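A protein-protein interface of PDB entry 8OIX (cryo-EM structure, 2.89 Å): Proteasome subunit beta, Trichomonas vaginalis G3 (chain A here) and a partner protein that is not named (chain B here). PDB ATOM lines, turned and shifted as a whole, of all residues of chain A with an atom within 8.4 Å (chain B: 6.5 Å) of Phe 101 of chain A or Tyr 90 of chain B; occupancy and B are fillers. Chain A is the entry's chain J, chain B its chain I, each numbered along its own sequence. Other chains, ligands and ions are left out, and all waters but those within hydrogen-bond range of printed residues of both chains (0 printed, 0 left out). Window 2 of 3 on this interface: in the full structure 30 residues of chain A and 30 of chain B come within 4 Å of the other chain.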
ATOM      1  N   LEU A  96     -14.452 -13.737  -0.083  1.00  0.00           N
ATOM      2  CA  LEU A  96     -15.258 -14.872   0.348  1.00  0.00           C
ATOM      3  C   LEU A  96     -14.437 -16.156   0.378  1.00  0.00           C
ATOM      4  O   LEU A  96     -14.604 -16.990   1.278  1.00  0.00           O
ATOM      5  CB  LEU A  96     -16.471 -15.025  -0.566  1.00  0.00           C
ATOM      6  CG  LEU A  96     -17.446 -13.847  -0.582  1.00  0.00           C
ATOM      7  CD1 LEU A  96     -18.600 -14.136  -1.516  1.00  0.00           C
ATOM      8  CD2 LEU A  96     -17.950 -13.532   0.815  1.00  0.00           C
ATOM      9  N   TYR A  97     -13.517 -16.334  -0.566  1.00  0.00           N
ATOM     10  CA  TYR A  97     -12.794 -17.593  -0.558  1.00  0.00           C
ATOM     11  C   TYR A  97     -11.688 -17.595   0.488  1.00  0.00           C
ATOM     12  O   TYR A  97     -11.224 -18.670   0.880  1.00  0.00           O
ATOM     13  CB  TYR A  97     -12.222 -17.907  -1.941  1.00  0.00           C
ATOM     14  CG  TYR A  97     -11.922 -19.378  -2.111  1.00  0.00           C
ATOM     15  CD1 TYR A  97     -12.888 -20.237  -2.613  1.00  0.00           C
ATOM     16  CD2 TYR A  97     -10.701 -19.915  -1.740  1.00  0.00           C
ATOM     17  CE1 TYR A  97     -12.639 -21.581  -2.761  1.00  0.00           C
ATOM     18  CE2 TYR A  97     -10.446 -21.264  -1.877  1.00  0.00           C
ATOM     19  CZ  TYR A  97     -11.417 -22.091  -2.395  1.00  0.00           C
ATOM     20  OH  TYR A  97     -11.167 -23.434  -2.541  1.00  0.00           O
ATOM     21  N   GLU A  98     -11.259 -16.423   0.961  1.00  0.00           N
ATOM     22  CA  GLU A  98     -10.335 -16.407   2.085  1.00  0.00           C
ATOM     23  C   GLU A  98     -10.995 -16.955   3.340  1.00  0.00           C
ATOM     24  O   GLU A  98     -10.298 -17.455   4.228  1.00  0.00           O
ATOM     25  CB  GLU A  98      -9.815 -14.990   2.334  1.00  0.00           C
ATOM     26  CG  GLU A  98      -8.751 -14.491   1.345  1.00  0.00           C
ATOM     27  CD  GLU A  98      -7.477 -15.326   1.313  1.00  0.00           C
ATOM     28  OE1 GLU A  98      -7.530 -16.519   0.945  1.00  0.00           O
ATOM     29  OE2 GLU A  98      -6.409 -14.778   1.655  1.00  0.00           O
ATOM     30  N   LYS A  99     -12.325 -16.873   3.427  1.00  0.00           N
ATOM     31  CA  LYS A  99     -13.088 -17.477   4.509  1.00  0.00           C
ATOM     32  C   LYS A  99     -13.864 -18.698   4.027  1.00  0.00           C
ATOM     33  O   LYS A  99     -14.796 -19.138   4.699  1.00  0.00           O
ATOM     34  CB  LYS A  99     -14.037 -16.455   5.131  1.00  0.00           C
ATOM     35  CG  LYS A  99     -13.371 -15.153   5.541  1.00  0.00           C
ATOM     36  CD  LYS A  99     -12.088 -15.378   6.317  1.00  0.00           C
ATOM     37  CE  LYS A  99     -11.368 -14.063   6.556  1.00  0.00           C
ATOM     38  NZ  LYS A  99     -10.000 -14.267   7.099  1.00  0.00           N
ATOM     39  N   ARG A 100     -13.486 -19.236   2.865  1.00  0.00           N
ATOM     40  CA  ARG A 100     -14.094 -20.435   2.284  1.00  0.00           C
ATOM     41  C   ARG A 100     -14.527 -21.482   3.307  1.00  0.00           C
ATOM     42  O   ARG A 100     -15.630 -22.029   3.215  1.00  0.00           O
ATOM     43  CB  ARG A 100     -13.094 -21.054   1.302  1.00  0.00           C
ATOM     44  CG  ARG A 100     -13.424 -22.446   0.800  1.00  0.00           C
ATOM     45  CD  ARG A 100     -14.736 -22.495   0.058  1.00  0.00           C
ATOM     46  NE  ARG A 100     -15.100 -23.856  -0.315  1.00  0.00           N
ATOM     47  CZ  ARG A 100     -15.363 -24.833   0.542  1.00  0.00           C
ATOM     48  NH1 ARG A 100     -15.529 -24.595   1.833  1.00  0.00           N
ATOM     49  NH2 ARG A 100     -15.526 -26.070   0.084  1.00  0.00           N
ATOM     50  N   PHE A 101     -13.675 -21.787   4.283  1.00  0.00           N
ATOM     51  CA  PHE A 101     -13.966 -22.868   5.215  1.00  0.00           C
ATOM     52  C   PHE A 101     -14.644 -22.393   6.493  1.00  0.00           C
ATOM     53  O   PHE A 101     -15.065 -23.228   7.299  1.00  0.00           O
ATOM     54  CB  PHE A 101     -12.682 -23.629   5.553  1.00  0.00           C
ATOM     55  CG  PHE A 101     -12.011 -24.231   4.354  1.00  0.00           C
ATOM     56  CD1 PHE A 101     -12.579 -25.311   3.700  1.00  0.00           C
ATOM     57  CD2 PHE A 101     -10.823 -23.714   3.873  1.00  0.00           C
ATOM     58  CE1 PHE A 101     -11.972 -25.866   2.594  1.00  0.00           C
ATOM     59  CE2 PHE A 101     -10.210 -24.266   2.767  1.00  0.00           C
ATOM     60  CZ  PHE A 101     -10.786 -25.343   2.127  1.00  0.00           C
ATOM     61  N   SER A 102     -14.764 -21.083   6.689  1.00  0.00           N
ATOM     62  CA  SER A 102     -15.671 -20.497   7.678  1.00  0.00           C
ATOM     63  C   SER A 102     -16.493 -19.425   6.974  1.00  0.00           C
ATOM     64  O   SER A 102     -16.398 -18.236   7.290  1.00  0.00           O
ATOM     65  CB  SER A 102     -14.896 -19.919   8.860  1.00  0.00           C
ATOM     66  OG  SER A 102     -13.938 -18.971   8.425  1.00  0.00           O
ATOM     67  N   PRO A 103     -17.308 -19.822   5.997  1.00  0.00           N
ATOM     68  CA  PRO A 103     -17.820 -18.854   5.020  1.00  0.00           C
ATOM     69  C   PRO A 103     -18.729 -17.804   5.631  1.00  0.00           C
ATOM     70  O   PRO A 103     -19.468 -18.060   6.584  1.00  0.00           O
ATOM     71  CB  PRO A 103     -18.588 -19.732   4.026  1.00  0.00           C
ATOM     72  CG  PRO A 103     -18.951 -20.946   4.798  1.00  0.00           C
ATOM     73  CD  PRO A 103     -17.830 -21.177   5.758  1.00  0.00           C
ATOM     74  N   PHE A 104     -18.659 -16.602   5.064  1.00  0.00           N
ATOM     75  CA  PHE A 104     -19.699 -15.617   5.302  1.00  0.00           C
ATOM     76  C   PHE A 104     -21.008 -16.159   4.755  1.00  0.00           C
ATOM     77  O   PHE A 104     -21.055 -16.682   3.639  1.00  0.00           O
ATOM     78  CB  PHE A 104     -19.361 -14.292   4.623  1.00  0.00           C
ATOM     79  CG  PHE A 104     -18.162 -13.599   5.191  1.00  0.00           C
ATOM     80  CD1 PHE A 104     -18.234 -12.946   6.408  1.00  0.00           C
ATOM     81  CD2 PHE A 104     -16.974 -13.559   4.485  1.00  0.00           C
ATOM     82  CE1 PHE A 104     -17.135 -12.294   6.922  1.00  0.00           C
ATOM     83  CE2 PHE A 104     -15.874 -12.904   4.993  1.00  0.00           C
ATOM     84  CZ  PHE A 104     -15.954 -12.273   6.214  1.00  0.00           C
ATOM     85  N   PHE A 105     -22.072 -16.035   5.534  1.00  0.00           N
ATOM     86  CA  PHE A 105     -23.371 -16.517   5.078  1.00  0.00           C
ATOM     87  C   PHE A 105     -24.132 -15.420   4.347  1.00  0.00           C
ATOM     88  O   PHE A 105     -25.269 -15.084   4.672  1.00  0.00           O
ATOM     89  CB  PHE A 105     -24.158 -17.067   6.258  1.00  0.00           C
ATOM     90  CG  PHE A 105     -23.390 -18.074   7.059  1.00  0.00           C
ATOM     91  CD1 PHE A 105     -23.247 -19.374   6.606  1.00  0.00           C
ATOM     92  CD2 PHE A 105     -22.795 -17.718   8.258  1.00  0.00           C
ATOM     93  CE1 PHE A 105     -22.530 -20.300   7.337  1.00  0.00           C
ATOM     94  CE2 PHE A 105     -22.078 -18.641   8.994  1.00  0.00           C
ATOM     95  CZ  PHE A 105     -21.947 -19.934   8.534  1.00  0.00           C
ATOM     96  N   SER A 127     -21.977 -18.155  -1.106  1.00  0.00           N
ATOM     97  CA  SER A 127     -21.327 -17.726   0.127  1.00  0.00           C
ATOM     98  C   SER A 127     -19.812 -17.644  -0.024  1.00  0.00           C
ATOM     99  O   SER A 127     -19.157 -16.891   0.706  1.00  0.00           O
ATOM    100  CB  SER A 127     -21.691 -18.680   1.264  1.00  0.00           C
ATOM    101  OG  SER A 127     -21.359 -20.016   0.932  1.00  0.00           O
ATOM    102  N   ILE A 128     -19.239 -18.401  -0.958  1.00  0.00           N
ATOM    103  CA  ILE A 128     -17.791 -18.562  -1.032  1.00  0.00           C
ATOM    104  C   ILE A 128     -17.237 -18.093  -2.371  1.00  0.00           C
ATOM    105  O   ILE A 128     -16.198 -18.582  -2.828  1.00  0.00           O
ATOM    106  CB  ILE A 128     -17.409 -20.027  -0.761  1.00  0.00           C
ATOM    107  CG1 ILE A 128     -18.280 -20.958  -1.603  1.00  0.00           C
ATOM    108  CG2 ILE A 128     -17.562 -20.351   0.708  1.00  0.00           C
ATOM    109  CD1 ILE A 128     -17.886 -22.407  -1.529  1.00  0.00           C
ATOM    110  N   ASP B  51     -14.586 -23.572  -5.268  1.00  0.00           N
ATOM    111  CA  ASP B  51     -13.348 -24.317  -5.069  1.00  0.00           C
ATOM    112  C   ASP B  51     -12.632 -24.541  -6.392  1.00  0.00           C
ATOM    113  O   ASP B  51     -11.420 -24.327  -6.498  1.00  0.00           O
ATOM    114  CB  ASP B  51     -13.646 -25.651  -4.387  1.00  0.00           C
ATOM    115  CG  ASP B  51     -13.966 -25.495  -2.918  1.00  0.00           C
ATOM    116  OD1 ASP B  51     -13.487 -24.521  -2.304  1.00  0.00           O
ATOM    117  OD2 ASP B  51     -14.693 -26.349  -2.375  1.00  0.00           O
ATOM    118  N   ILE B  55      -9.044 -22.779  -7.132  1.00  0.00           N
ATOM    119  CA  ILE B  55      -7.862 -23.626  -7.246  1.00  0.00           C
ATOM    120  C   ILE B  55      -7.283 -23.539  -8.649  1.00  0.00           C
ATOM    121  O   ILE B  55      -6.061 -23.548  -8.829  1.00  0.00           O
ATOM    122  CB  ILE B  55      -8.170 -25.078  -6.835  1.00  0.00           C
ATOM    123  CG1 ILE B  55      -6.863 -25.833  -6.604  1.00  0.00           C
ATOM    124  CG2 ILE B  55      -9.007 -25.797  -7.882  1.00  0.00           C
ATOM    125  CD1 ILE B  55      -7.048 -27.239  -6.132  1.00  0.00           C
ATOM    126  N   SER B  85      -1.396 -32.299  -4.833  1.00  0.00           N
ATOM    127  CA  SER B  85      -0.833 -31.971  -3.530  1.00  0.00           C
ATOM    128  C   SER B  85      -1.694 -30.948  -2.805  1.00  0.00           C
ATOM    129  O   SER B  85      -1.945 -31.080  -1.601  1.00  0.00           O
ATOM    130  CB  SER B  85       0.596 -31.458  -3.690  1.00  0.00           C
ATOM    131  OG  SER B  85       0.618 -30.224  -4.385  1.00  0.00           O
ATOM    132  N   ARG B  86      -2.169 -29.924  -3.521  1.00  0.00           N
ATOM    133  CA  ARG B  86      -3.012 -28.919  -2.882  1.00  0.00           C
ATOM    134  C   ARG B  86      -4.332 -29.520  -2.414  1.00  0.00           C
ATOM    135  O   ARG B  86      -4.804 -29.213  -1.316  1.00  0.00           O
ATOM    136  CB  ARG B  86      -3.260 -27.752  -3.834  1.00  0.00           C
ATOM    137  CG  ARG B  86      -4.167 -26.686  -3.252  1.00  0.00           C
ATOM    138  CD  ARG B  86      -4.171 -25.426  -4.091  1.00  0.00           C
ATOM    139  NE  ARG B  86      -5.047 -24.411  -3.519  1.00  0.00           N
ATOM    140  CZ  ARG B  86      -4.693 -23.580  -2.549  1.00  0.00           C
ATOM    141  NH1 ARG B  86      -3.478 -23.607  -2.025  1.00  0.00           N
ATOM    142  NH2 ARG B  86      -5.579 -22.699  -2.095  1.00  0.00           N
ATOM    143  N   LEU B  87      -4.938 -30.388  -3.227  1.00  0.00           N
ATOM    144  CA  LEU B  87      -6.206 -30.997  -2.841  1.00  0.00           C
ATOM    145  C   LEU B  87      -6.028 -32.006  -1.718  1.00  0.00           C
ATOM    146  O   LEU B  87      -6.945 -32.200  -0.912  1.00  0.00           O
ATOM    147  CB  LEU B  87      -6.863 -31.657  -4.052  1.00  0.00           C
ATOM    148  CG  LEU B  87      -7.436 -30.694  -5.088  1.00  0.00           C
ATOM    149  CD1 LEU B  87      -7.856 -31.427  -6.338  1.00  0.00           C
ATOM    150  CD2 LEU B  87      -8.617 -29.969  -4.495  1.00  0.00           C
ATOM    151  N   PHE B  88      -4.870 -32.663  -1.651  1.00  0.00           N
ATOM    152  CA  PHE B  88      -4.606 -33.583  -0.553  1.00  0.00           C
ATOM    153  C   PHE B  88      -4.366 -32.832   0.748  1.00  0.00           C
ATOM    154  O   PHE B  88      -4.837 -33.255   1.811  1.00  0.00           O
ATOM    155  CB  PHE B  88      -3.407 -34.467  -0.888  1.00  0.00           C
ATOM    156  CG  PHE B  88      -3.144 -35.531   0.131  1.00  0.00           C
ATOM    157  CD1 PHE B  88      -3.828 -36.730   0.085  1.00  0.00           C
ATOM    158  CD2 PHE B  88      -2.226 -35.326   1.146  1.00  0.00           C
ATOM    159  CE1 PHE B  88      -3.595 -37.708   1.022  1.00  0.00           C
ATOM    160  CE2 PHE B  88      -1.994 -36.300   2.090  1.00  0.00           C
ATOM    161  CZ  PHE B  88      -2.678 -37.494   2.027  1.00  0.00           C
ATOM    162  N   GLN B  89      -3.632 -31.717   0.690  1.00  0.00           N
ATOM    163  CA  GLN B  89      -3.368 -30.949   1.899  1.00  0.00           C
ATOM    164  C   GLN B  89      -4.630 -30.317   2.468  1.00  0.00           C
ATOM    165  O   GLN B  89      -4.639 -29.934   3.641  1.00  0.00           O
ATOM    166  CB  GLN B  89      -2.317 -29.871   1.627  1.00  0.00           C
ATOM    167  CG  GLN B  89      -0.932 -30.414   1.287  1.00  0.00           C
ATOM    168  CD  GLN B  89      -0.431 -31.455   2.278  1.00  0.00           C
ATOM    169  OE1 GLN B  89      -0.727 -31.394   3.472  1.00  0.00           O
ATOM    170  NE2 GLN B  89       0.330 -32.423   1.779  1.00  0.00           N
ATOM    171  N   TYR B  90      -5.689 -30.203   1.670  1.00  0.00           N
ATOM    172  CA  TYR B  90      -6.991 -29.782   2.162  1.00  0.00           C
ATOM    173  C   TYR B  90      -7.928 -30.956   2.404  1.00  0.00           C
ATOM    174  O   TYR B  90      -9.114 -30.745   2.668  1.00  0.00           O
ATOM    175  CB  TYR B  90      -7.623 -28.780   1.194  1.00  0.00           C
ATOM    176  CG  TYR B  90      -6.953 -27.427   1.232  1.00  0.00           C
ATOM    177  CD1 TYR B  90      -7.100 -26.592   2.329  1.00  0.00           C
ATOM    178  CD2 TYR B  90      -6.162 -26.991   0.180  1.00  0.00           C
ATOM    179  CE1 TYR B  90      -6.485 -25.359   2.373  1.00  0.00           C
ATOM    180  CE2 TYR B  90      -5.545 -25.759   0.215  1.00  0.00           C
ATOM    181  CZ  TYR B  90      -5.708 -24.947   1.314  1.00  0.00           C
ATOM    182  OH  TYR B  90      -5.094 -23.718   1.353  1.00  0.00           O
ATOM    183  N   MET B  91      -7.417 -32.186   2.311  1.00  0.00           N
ATOM    184  CA  MET B  91      -8.128 -33.388   2.751  1.00  0.00           C
ATOM    185  C   MET B  91      -9.497 -33.516   2.090  1.00  0.00           C
ATOM    186  O   MET B  91     -10.464 -33.981   2.697  1.00  0.00           O
ATOM    187  CB  MET B  91      -8.257 -33.411   4.274  1.00  0.00           C
ATOM    188  CG  MET B  91      -6.927 -33.483   5.003  1.00  0.00           C
ATOM    189  SD  MET B  91      -6.967 -32.665   6.606  1.00  0.00           S
ATOM    190  CE  MET B  91      -7.090 -30.950   6.103  1.00  0.00           C
ATOM    191  N   GLY B  92      -9.582 -33.102   0.830  1.00  0.00           N
ATOM    192  CA  GLY B  92     -10.818 -33.204   0.088  1.00  0.00           C
ATOM    193  C   GLY B  92     -11.846 -32.137   0.385  1.00  0.00           C
ATOM    194  O   GLY B  92     -12.956 -32.208  -0.156  1.00  0.00           O
ATOM    195  N   TYR B  93     -11.523 -31.153   1.227  1.00  0.00           N
ATOM    196  CA  TYR B  93     -12.486 -30.103   1.532  1.00  0.00           C
ATOM    197  C   TYR B  93     -12.627 -29.113   0.386  1.00  0.00           C
ATOM    198  O   TYR B  93     -13.687 -28.495   0.234  1.00  0.00           O
ATOM    199  CB  TYR B  93     -12.094 -29.382   2.821  1.00  0.00           C
ATOM    200  CG  TYR B  93     -12.114 -30.279   4.036  1.00  0.00           C
ATOM    201  CD1 TYR B  93     -13.170 -31.151   4.259  1.00  0.00           C
ATOM    202  CD2 TYR B  93     -11.078 -30.257   4.959  1.00  0.00           C
ATOM    203  CE1 TYR B  93     -13.194 -31.975   5.365  1.00  0.00           C
ATOM    204  CE2 TYR B  93     -11.093 -31.078   6.069  1.00  0.00           C
ATOM    205  CZ  TYR B  93     -12.154 -31.934   6.266  1.00  0.00           C
ATOM    206  OH  TYR B  93     -12.174 -32.754   7.371  1.00  0.00           O
ATOM    207  N   ILE B  94     -11.584 -28.946  -0.424  1.00  0.00           N
ATOM    208  CA  ILE B  94     -11.716 -28.223  -1.683  1.00  0.00           C
ATOM    209  C   ILE B  94     -12.307 -29.197  -2.692  1.00  0.00           C
ATOM    210  O   ILE B  94     -11.583 -29.963  -3.336  1.00  0.00           O
ATOM    211  CB  ILE B  94     -10.373 -27.641  -2.160  1.00  0.00           C
ATOM    212  CG1 ILE B  94      -9.905 -26.545  -1.204  1.00  0.00           C
ATOM    213  CG2 ILE B  94     -10.501 -27.065  -3.561  1.00  0.00           C
ATOM    214  CD1 ILE B  94      -8.750 -25.726  -1.735  1.00  0.00           C
ATOM    215  N   PRO B 115     -11.096 -34.629  -5.683  1.00  0.00           N
ATOM    216  CA  PRO B 115     -11.059 -33.580  -4.651  1.00  0.00           C
ATOM    217  C   PRO B 115     -10.131 -33.905  -3.495  1.00  0.00           C
ATOM    218  O   PRO B 115      -9.616 -32.984  -2.850  1.00  0.00           O
ATOM    219  CB  PRO B 115     -12.520 -33.487  -4.195  1.00  0.00           C
ATOM    220  CG  PRO B 115     -13.301 -33.951  -5.366  1.00  0.00           C
ATOM    221  CD  PRO B 115     -12.479 -35.020  -6.015  1.00  0.00           C
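Printed residues of chain B that touch a printed residue of chain A: Asp 51, Tyr 90, Tyr 93 and Ile 94. Hydrophobic or aromatic side chains of chain B that line the printed part of chain A: Tyr 90, Tyr 93 and Ile 94. Among the printed residues, 7 pairs touch across the chains. Among the printed residues, Asp or Glu carboxylates within 4 Å of a Lys or Arg side-chain nitrogen of the other chain: Arg 100 of chain A with Asp 51 of chain B (2.6 Å).
Tyr 90 of chain B touches just one residue of chain A: Phe 101. Printed residues of chain A within 4 Å of Asp 51 of chain B: Tyr 97 and Arg 100. Printed residues of chain B within 4 Å of Tyr 97 of chain A: Asp 51 (2.6 Å) and Ile 94 (3.4 Å). Of the printed residues of chain B, Arg 100 of chain A touches Asp 51 and Tyr 93. Printed residues of chain A within 4 Å of Tyr 93 of chain B: Arg 100 (3.0 Å) and Phe 101 (3.5 Å). Of the printed residues of chain A, Ile 94 of chain B touches Tyr 97 (3.4 Å) and Phe 101 (3.6 Å). Leu 87 of chain B touches none of the printed residues of chain A. Glu 98 of chain A touches none of the printed residues of chain B.
OH of Tyr 97 of chain A sits at hydrogen-bond distance from OD1 of Asp 51 of chain B, 2.6 Å away. The guanidinium group (NH2) of Arg 100 of chain A lies within salt-bridge range of the side-chain carboxylate (OD2) of Asp 51 of chain B, 2.6 Å away. The guanidinium group (NH2) of Arg 100 of chain A is in hydrogen-bond range of the backbone carbonyl oxygen (O) of Tyr 93 of chain B (3.0 Å).
Among the printed residues, merely in contact across the chains: Tyr 97 of chain A with Ile 94 of chain B, Phe 101 of chain A with Tyr 90 of chain B, Phe 101 of chain A with Tyr 93 of chain B and Phe 101 of chain A with Ile 94 of chain B.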
